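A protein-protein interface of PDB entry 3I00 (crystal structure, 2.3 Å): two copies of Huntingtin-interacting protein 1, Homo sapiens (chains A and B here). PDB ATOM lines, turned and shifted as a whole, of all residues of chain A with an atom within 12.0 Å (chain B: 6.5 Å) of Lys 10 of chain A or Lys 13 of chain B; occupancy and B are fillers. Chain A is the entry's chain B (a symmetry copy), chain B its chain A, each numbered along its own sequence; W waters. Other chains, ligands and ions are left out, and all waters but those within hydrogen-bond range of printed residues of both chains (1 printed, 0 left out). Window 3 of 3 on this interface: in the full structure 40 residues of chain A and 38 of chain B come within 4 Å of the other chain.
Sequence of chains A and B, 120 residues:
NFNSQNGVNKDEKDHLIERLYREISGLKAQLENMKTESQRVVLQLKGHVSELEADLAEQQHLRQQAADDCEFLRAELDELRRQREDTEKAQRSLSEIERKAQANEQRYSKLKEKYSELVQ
Lys 10 of chain A touches just one residue of chain B: Lys 13 (3.9 Å). Printed residues of chain B within 4 Å of Lys 13 of chain A: Lys 10 (2.2 Å), Lys 13 (3.95 Å) and Asp 14 (2.8 Å). Printed residues of chain B within 4 Å of Leu 16 of chain A: Ile 17 (3.8 Å). Of the printed residues of chain B, Leu 20 of chain A touches Ile 17. Asp 11 of chain B touches none of the printed residues of chain A. No residue of chain A comes within 4 Å of Glu 12 of chain B. Of chain A, only Lys 10 (3.9 Å), Lys 13 (3.95 Å), Asp 14 (2.9 Å) and Ile 17 (3.9 Å) come within 4 Å of Lys 13 of chain B. Of chain A, only Lys 13 (2.8 Å) comes within 4 Å of Asp 14 of chain B. No residue of chain A comes within 4 Å of His 15 of chain B. Leu 16 of chain B touches two residues of chain A. Ile 17 of chain B touches three residues of chain A. The nearest residue of chain B that does not touch Lys 10 of chain A is Lys 10 of chain B (4.3 Å).
Printed residues of chain B that touch a printed residue of chain A: Lys 10, Lys 13, Asp 14, Leu 16 and Ile 17. Hydrophobic or aromatic side chains of chain B within 4 Å of the printed part of chain A: Leu 16 and Ile 17. Of the 15 printed residues of chain A, 7 touch a printed residue of chain B. Hydrophobic or aromatic side chains of chain A that line the printed part of chain B: Leu 16, Ile 17, Leu 20 and Tyr 21. Among the printed residues, Asp or Glu carboxylates within 4 Å of a Lys or Arg side-chain nitrogen of the other chain: Lys 13 of chain A with Asp 14 of chain B (2.8 Å) and Asp 14 of chain A with Lys 13 of chain B (2.9 Å).
Lys 10 of chain A touches Lys 13 of chain B, and with the chains exchanged Lys 13 of chain A touches Lys 10 of chain B. Lys 13 of chain A touches Asp 14 of chain B, and with the chains exchanged Asp 14 of chain A touches Lys 13 of chain B. Leu 16 of chain A touches Ile 17 of chain B, and with the chains exchanged Ile 17 of chain A touches Leu 16 of chain B. Ile 17 of chain B touches its own counterpart, Ile 17 of chain A. Of the 11 pairs that touch across the chains among the printed residues, 8 have their exchanged pair printed and touching as well.
Water W1 lies within hydrogen-bond range of the side-chain amino group of Lys 13 of chain A, the backbone NH of Lys 10 of chain B and the backbone carbonyl oxygen of Val 8 of chain A.
Among the printed residues, pairs that only touch across the chains: Lys 10 of chain A with Lys 13 of chain B (3.9 Å), Lys 13 of chain A with Lys 13 of chain B (3.95 Å), Leu 16 of chain A with Ile 17 of chain B (3.8 Å), Ile 17 of chain A with Lys 13 of chain B (3.9 Å), Ile 17 of chain A with Leu 16 of chain B (3.9 Å), Ile 17 of chain A with Ile 17 of chain B (3.5 Å), Leu 20 of chain A with Ile 17 of chain B (3.4 Å) and Tyr 21 of chain A with Leu 16 of chain B (3.8 Å).
The side-chain amino group of Lys 13 of chain B lies within salt-bridge range of the side-chain carboxylate of Asp 14 of chain A (2.9 Å). NZ of Lys 13 of chain A is in salt-bridge range of OD2 of Asp 14 of chain B. The backbone carbonyl oxygen (O) of Lys 10 of chain B sits close to the side-chain amino group (NZ) of Lys 13 of chain A, 2.2 Å away.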
ATOM      1  N   GLY A   7      23.780  21.287 -30.304  1.00  0.00           N
ATOM      2  CA  GLY A   7      24.125  22.334 -29.280  1.00  0.00           C
ATOM      3  C   GLY A   7      23.962  21.755 -27.883  1.00  0.00           C
ATOM      4  O   GLY A   7      24.729  20.864 -27.482  1.00  0.00           O
ATOM      5  N   VAL A   8      22.953  22.251 -27.154  1.00  0.00           N
ATOM      6  CA  VAL A   8      22.533  21.688 -25.849  1.00  0.00           C
ATOM      7  C   VAL A   8      22.468  20.155 -25.850  1.00  0.00           C
ATOM      8  O   VAL A   8      22.606  19.527 -24.791  1.00  0.00           O
ATOM      9  CB  VAL A   8      21.189  22.286 -25.419  1.00  0.00           C
ATOM     10  N   ASN A   9      22.193  19.602 -27.037  1.00  0.00           N
ATOM     11  CA  ASN A   9      22.468  18.214 -27.490  1.00  0.00           C
ATOM     12  C   ASN A   9      21.447  17.831 -28.567  1.00  0.00           C
ATOM     13  O   ASN A   9      21.204  16.643 -28.839  1.00  0.00           O
ATOM     14  CB  ASN A   9      22.524  17.163 -26.360  1.00  0.00           C
ATOM     15  CG  ASN A   9      23.962  16.850 -25.897  1.00  0.00           C
ATOM     16  OD1 ASN A   9      24.214  16.706 -24.705  1.00  0.00           O
ATOM     17  ND2 ASN A   9      24.899  16.754 -26.842  1.00  0.00           N
ATOM     18  N   LYS A  10      20.887  18.869 -29.190  1.00  0.00           N
ATOM     19  CA  LYS A  10      19.691  18.782 -30.029  1.00  0.00           C
ATOM     20  C   LYS A  10      19.817  17.854 -31.244  1.00  0.00           C
ATOM     21  O   LYS A  10      18.940  17.017 -31.470  1.00  0.00           O
ATOM     22  CB  LYS A  10      19.260  20.192 -30.446  1.00  0.00           C
ATOM     23  CG  LYS A  10      18.140  20.255 -31.473  1.00  0.00           C
ATOM     24  CD  LYS A  10      17.844  21.706 -31.843  1.00  0.00           C
ATOM     25  CE  LYS A  10      17.145  21.822 -33.192  1.00  0.00           C
ATOM     26  NZ  LYS A  10      15.788  21.206 -33.216  1.00  0.00           N
ATOM     27  N   ASP A  11      20.900  18.004 -32.012  1.00  0.00           N
ATOM     28  CA  ASP A  11      21.145  17.174 -33.204  1.00  0.00           C
ATOM     29  C   ASP A  11      21.415  15.712 -32.884  1.00  0.00           C
ATOM     30  O   ASP A  11      20.875  14.829 -33.538  1.00  0.00           O
ATOM     31  CB  ASP A  11      22.283  17.746 -34.051  1.00  0.00           C
ATOM     32  CG  ASP A  11      21.846  18.948 -34.879  1.00  0.00           C
ATOM     33  OD1 ASP A  11      22.618  19.928 -34.973  1.00  0.00           O
ATOM     34  OD2 ASP A  11      20.725  18.914 -35.434  1.00  0.00           O
ATOM     35  N   GLU A  12      22.241  15.472 -31.868  1.00  0.00           N
ATOM     36  CA  GLU A  12      22.560  14.124 -31.374  1.00  0.00           C
ATOM     37  C   GLU A  12      21.309  13.296 -31.031  1.00  0.00           C
ATOM     38  O   GLU A  12      21.297  12.071 -31.200  1.00  0.00           O
ATOM     39  CB  GLU A  12      23.489  14.214 -30.151  1.00  0.00           C
ATOM     40  CG  GLU A  12      24.886  14.798 -30.444  1.00  0.00           C
ATOM     41  CD  GLU A  12      24.928  16.331 -30.535  1.00  0.00           C
ATOM     42  OE1 GLU A  12      23.868  17.000 -30.454  1.00  0.00           O
ATOM     43  OE2 GLU A  12      26.045  16.872 -30.689  1.00  0.00           O
ATOM     44  N   LYS A  13      20.267  13.982 -30.561  1.00  0.00           N
ATOM     45  CA  LYS A  13      18.992  13.357 -30.225  1.00  0.00           C
ATOM     46  C   LYS A  13      18.128  13.149 -31.461  1.00  0.00           C
ATOM     47  O   LYS A  13      17.461  12.122 -31.585  1.00  0.00           O
ATOM     48  CB  LYS A  13      18.233  14.188 -29.199  1.00  0.00           C
ATOM     49  CG  LYS A  13      18.973  14.409 -27.910  1.00  0.00           C
ATOM     50  CD  LYS A  13      18.079  15.099 -26.925  1.00  0.00           C
ATOM     51  CE  LYS A  13      18.890  15.777 -25.852  1.00  0.00           C
ATOM     52  NZ  LYS A  13      18.064  15.997 -24.639  1.00  0.00           N
ATOM     53  N   ASP A  14      18.133  14.127 -32.367  1.00  0.00           N
ATOM     54  CA  ASP A  14      17.542  13.961 -33.684  1.00  0.00           C
ATOM     55  C   ASP A  14      18.218  12.816 -34.451  1.00  0.00           C
ATOM     56  O   ASP A  14      17.537  12.023 -35.105  1.00  0.00           O
ATOM     57  CB  ASP A  14      17.636  15.261 -34.481  1.00  0.00           C
ATOM     58  CG  ASP A  14      16.575  16.283 -34.078  1.00  0.00           C
ATOM     59  OD1 ASP A  14      15.554  15.886 -33.471  1.00  0.00           O
ATOM     60  OD2 ASP A  14      16.758  17.484 -34.391  1.00  0.00           O
ATOM     61  N   HIS A  15      19.548  12.725 -34.355  1.00  0.00           N
ATOM     62  CA  HIS A  15      20.283  11.620 -34.967  1.00  0.00           C
ATOM     63  C   HIS A  15      19.761  10.274 -34.454  1.00  0.00           C
ATOM     64  O   HIS A  15      19.401   9.405 -35.249  1.00  0.00           O
ATOM     65  CB  HIS A  15      21.797  11.751 -34.727  1.00  0.00           C
ATOM     66  CG  HIS A  15      22.592  10.538 -35.134  1.00  0.00           C
ATOM     67  ND1 HIS A  15      23.206  10.422 -36.364  1.00  0.00           N
ATOM     68  CD2 HIS A  15      22.882   9.393 -34.467  1.00  0.00           C
ATOM     69  CE1 HIS A  15      23.838   9.264 -36.438  1.00  0.00           C
ATOM     70  NE2 HIS A  15      23.657   8.618 -35.301  1.00  0.00           N
ATOM     71  N   LEU A  16      19.711  10.113 -33.131  1.00  0.00           N
ATOM     72  CA  LEU A  16      19.268   8.860 -32.522  1.00  0.00           C
ATOM     73  C   LEU A  16      17.819   8.571 -32.855  1.00  0.00           C
ATOM     74  O   LEU A  16      17.472   7.455 -33.224  1.00  0.00           O
ATOM     75  CB  LEU A  16      19.471   8.877 -30.999  1.00  0.00           C
ATOM     76  CG  LEU A  16      18.891   7.705 -30.200  1.00  0.00           C
ATOM     77  CD1 LEU A  16      19.609   6.392 -30.574  1.00  0.00           C
ATOM     78  CD2 LEU A  16      18.952   7.958 -28.695  1.00  0.00           C
ATOM     79  N   ILE A  17      16.975   9.588 -32.758  1.00  0.00           N
ATOM     80  CA  ILE A  17      15.581   9.400 -33.079  1.00  0.00           C
ATOM     81  C   ILE A  17      15.426   8.746 -34.452  1.00  0.00           C
ATOM     82  O   ILE A  17      14.627   7.821 -34.617  1.00  0.00           O
ATOM     83  CB  ILE A  17      14.774  10.714 -32.903  1.00  0.00           C
ATOM     84  CG1 ILE A  17      14.550  10.959 -31.398  1.00  0.00           C
ATOM     85  CG2 ILE A  17      13.447  10.663 -33.647  1.00  0.00           C
ATOM     86  CD1 ILE A  17      14.111  12.410 -31.019  1.00  0.00           C
ATOM     87  N   GLU A  18      16.219   9.202 -35.419  1.00  0.00           N
ATOM     88  CA  GLU A  18      16.143   8.689 -36.773  1.00  0.00           C
ATOM     89  C   GLU A  18      16.543   7.223 -36.799  1.00  0.00           C
ATOM     90  O   GLU A  18      15.864   6.402 -37.395  1.00  0.00           O
ATOM     91  CB  GLU A  18      17.004   9.522 -37.736  1.00  0.00           C
ATOM     92  CG  GLU A  18      17.152   8.909 -39.123  1.00  0.00           C
ATOM     93  CD  GLU A  18      15.822   8.633 -39.821  1.00  0.00           C
ATOM     94  OE1 GLU A  18      14.866   9.442 -39.703  1.00  0.00           O
ATOM     95  OE2 GLU A  18      15.735   7.601 -40.512  1.00  0.00           O
ATOM     96  N   ARG A  19      17.632   6.898 -36.124  1.00  0.00           N
ATOM     97  CA  ARG A  19      18.099   5.513 -36.041  1.00  0.00           C
ATOM     98  C   ARG A  19      17.026   4.604 -35.448  1.00  0.00           C
ATOM     99  O   ARG A  19      16.863   3.456 -35.902  1.00  0.00           O
ATOM    100  CB  ARG A  19      19.403   5.416 -35.222  1.00  0.00           C
ATOM    101  CG  ARG A  19      20.611   6.159 -35.840  1.00  0.00           C
ATOM    102  CD  ARG A  19      20.726   5.858 -37.325  1.00  0.00           C
ATOM    103  NE  ARG A  19      21.678   6.695 -38.076  1.00  0.00           N
ATOM    104  CZ  ARG A  19      21.486   7.968 -38.421  1.00  0.00           C
ATOM    105  NH1 ARG A  19      20.387   8.617 -38.042  1.00  0.00           N
ATOM    106  NH2 ARG A  19      22.417   8.602 -39.127  1.00  0.00           N
ATOM    107  N   LEU A  20      16.294   5.118 -34.455  1.00  0.00           N
ATOM    108  CA  LEU A  20      15.219   4.361 -33.790  1.00  0.00           C
ATOM    109  C   LEU A  20      14.004   4.204 -34.702  1.00  0.00           C
ATOM    110  O   LEU A  20      13.405   3.132 -34.748  1.00  0.00           O
ATOM    111  CB  LEU A  20      14.830   4.995 -32.447  1.00  0.00           C
ATOM    112  CG  LEU A  20      15.932   5.133 -31.376  1.00  0.00           C
ATOM    113  CD1 LEU A  20      15.372   5.769 -30.099  1.00  0.00           C
ATOM    114  CD2 LEU A  20      16.647   3.806 -31.078  1.00  0.00           C
ATOM    115  N   TYR A  21      13.659   5.254 -35.448  1.00  0.00           N
ATOM    116  CA  TYR A  21      12.677   5.128 -36.521  1.00  0.00           C
ATOM    117  C   TYR A  21      13.034   3.959 -37.474  1.00  0.00           C
ATOM    118  O   TYR A  21      12.168   3.143 -37.817  1.00  0.00           O
ATOM    119  CB  TYR A  21      12.528   6.442 -37.311  1.00  0.00           C
ATOM    120  CG  TYR A  21      11.805   7.577 -36.580  1.00  0.00           C
ATOM    121  CD1 TYR A  21      10.849   7.319 -35.593  1.00  0.00           C
ATOM    122  CD2 TYR A  21      12.050   8.908 -36.912  1.00  0.00           C
ATOM    123  CE1 TYR A  21      10.171   8.357 -34.937  1.00  0.00           C
ATOM    124  CE2 TYR A  21      11.373   9.956 -36.271  1.00  0.00           C
ATOM    125  CZ  TYR A  21      10.441   9.669 -35.278  1.00  0.00           C
ATOM    126  OH  TYR A  21       9.786  10.695 -34.633  1.00  0.00           O
ATOM    127  N   LYS B  10      17.986  19.866 -25.381  1.00  0.00           N
ATOM    128  CA  LYS B  10      16.608  19.388 -25.724  1.00  0.00           C
ATOM    129  C   LYS B  10      16.042  18.485 -24.633  1.00  0.00           C
ATOM    130  O   LYS B  10      16.778  17.697 -24.031  1.00  0.00           O
ATOM    131  CB  LYS B  10      16.619  18.655 -27.057  1.00  0.00           C
ATOM    132  N   ASP B  11      14.747  18.612 -24.352  1.00  0.00           N
ATOM    133  CA  ASP B  11      14.090  17.625 -23.505  1.00  0.00           C
ATOM    134  C   ASP B  11      13.120  16.792 -24.320  1.00  0.00           C
ATOM    135  O   ASP B  11      13.544  15.803 -24.869  1.00  0.00           O
ATOM    136  CB  ASP B  11      13.424  18.230 -22.266  1.00  0.00           C
ATOM    137  CG  ASP B  11      13.075  17.169 -21.226  1.00  0.00           C
ATOM    138  OD1 ASP B  11      13.643  17.199 -20.115  1.00  0.00           O
ATOM    139  OD2 ASP B  11      12.251  16.282 -21.531  1.00  0.00           O
ATOM    140  N   GLU B  12      11.852  17.210 -24.413  1.00  0.00           N
ATOM    141  CA  GLU B  12      10.751  16.467 -25.079  1.00  0.00           C
ATOM    142  C   GLU B  12      11.140  15.357 -26.070  1.00  0.00           C
ATOM    143  O   GLU B  12      10.443  14.337 -26.171  1.00  0.00           O
ATOM    144  CB  GLU B  12       9.768  17.445 -25.741  1.00  0.00           C
ATOM    145  CG  GLU B  12       8.436  16.836 -26.197  1.00  0.00           C
ATOM    146  CD  GLU B  12       7.512  16.450 -25.042  1.00  0.00           C
ATOM    147  OE1 GLU B  12       7.777  15.422 -24.368  1.00  0.00           O
ATOM    148  OE2 GLU B  12       6.507  17.165 -24.826  1.00  0.00           O
ATOM    149  N   LYS B  13      12.226  15.582 -26.814  1.00  0.00           N
ATOM    150  CA  LYS B  13      12.927  14.533 -27.570  1.00  0.00           C
ATOM    151  C   LYS B  13      13.297  13.374 -26.638  1.00  0.00           C
ATOM    152  O   LYS B  13      13.051  12.220 -26.961  1.00  0.00           O
ATOM    153  CB  LYS B  13      14.195  15.098 -28.225  1.00  0.00           C
ATOM    154  CG  LYS B  13      13.955  16.277 -29.169  1.00  0.00           C
ATOM    155  CD  LYS B  13      15.236  16.679 -29.873  1.00  0.00           C
ATOM    156  CE  LYS B  13      15.092  18.007 -30.605  1.00  0.00           C
ATOM    157  NZ  LYS B  13      14.204  17.889 -31.793  1.00  0.00           N
ATOM    158  N   ASP B  14      13.874  13.700 -25.480  1.00  0.00           N
ATOM    159  CA  ASP B  14      14.192  12.725 -24.434  1.00  0.00           C
ATOM    160  C   ASP B  14      13.030  11.791 -24.118  1.00  0.00           C
ATOM    161  O   ASP B  14      13.235  10.598 -23.915  1.00  0.00           O
ATOM    162  CB  ASP B  14      14.658  13.435 -23.156  1.00  0.00           C
ATOM    163  CG  ASP B  14      16.119  13.877 -23.219  1.00  0.00           C
ATOM    164  OD1 ASP B  14      16.935  13.207 -23.891  1.00  0.00           O
ATOM    165  OD2 ASP B  14      16.462  14.884 -22.570  1.00  0.00           O
ATOM    166  N   HIS B  15      11.813  12.327 -24.082  1.00  0.00           N
ATOM    167  CA  HIS B  15      10.642  11.514 -23.755  1.00  0.00           C
ATOM    168  C   HIS B  15      10.152  10.700 -24.950  1.00  0.00           C
ATOM    169  O   HIS B  15       9.515   9.660 -24.777  1.00  0.00           O
ATOM    170  CB  HIS B  15       9.509  12.365 -23.162  1.00  0.00           C
ATOM    171  CG  HIS B  15       9.814  12.916 -21.802  1.00  0.00           C
ATOM    172  ND1 HIS B  15      10.153  12.116 -20.730  1.00  0.00           N
ATOM    173  CD2 HIS B  15       9.811  14.188 -21.334  1.00  0.00           C
ATOM    174  CE1 HIS B  15      10.357  12.872 -19.665  1.00  0.00           C
ATOM    175  NE2 HIS B  15      10.156  14.132 -20.005  1.00  0.00           N
ATOM    176  N   LEU B  16      10.455  11.179 -26.156  1.00  0.00           N
ATOM    177  CA  LEU B  16      10.134  10.465 -27.387  1.00  0.00           C
ATOM    178  C   LEU B  16      11.043   9.258 -27.504  1.00  0.00           C
ATOM    179  O   LEU B  16      10.733   8.295 -28.195  1.00  0.00           O
ATOM    180  CB  LEU B  16      10.359  11.374 -28.599  1.00  0.00           C
ATOM    181  CG  LEU B  16       9.479  11.327 -29.861  1.00  0.00           C
ATOM    182  CD1 LEU B  16      10.277  11.835 -31.054  1.00  0.00           C
ATOM    183  CD2 LEU B  16       8.895   9.967 -30.182  1.00  0.00           C
ATOM    184  N   ILE B  17      12.157   9.307 -26.785  1.00  0.00           N
ATOM    185  CA  ILE B  17      13.271   8.401 -27.013  1.00  0.00           C
ATOM    186  C   ILE B  17      13.297   6.937 -26.533  1.00  0.00           C
ATOM    187  O   ILE B  17      13.274   6.090 -27.391  1.00  0.00           O
ATOM    188  CB  ILE B  17      14.656   9.104 -26.795  1.00  0.00           C
ATOM    189  CG1 ILE B  17      15.062   9.849 -28.079  1.00  0.00           C
ATOM    190  CG2 ILE B  17      15.742   8.115 -26.419  1.00  0.00           C
ATOM    191  CD1 ILE B  17      16.379  10.640 -27.999  1.00  0.00           C
ATOM    192  N   GLU B  18      13.251   6.548 -25.261  1.00  0.00           N
ATOM    193  CA  GLU B  18      12.168   6.651 -24.246  1.00  0.00           C
ATOM    194  C   GLU B  18      10.884   5.941 -24.730  1.00  0.00           C
ATOM    195  O   GLU B  18      10.748   4.732 -24.500  1.00  0.00           O
ATOM    196  CB  GLU B  18      11.988   7.981 -23.518  1.00  0.00           C
ATOM    197  CG  GLU B  18      12.623   7.960 -22.084  1.00  0.00           C
ATOM    198  CD  GLU B  18      11.772   8.612 -20.994  1.00  0.00           C
ATOM    199  OE1 GLU B  18      10.593   8.226 -20.813  1.00  0.00           O
ATOM    200  OE2 GLU B  18      12.302   9.485 -20.268  1.00  0.00           O
HETATM  201  O   HOH W   1      19.529  18.108 -23.916  1.00  0.00           O
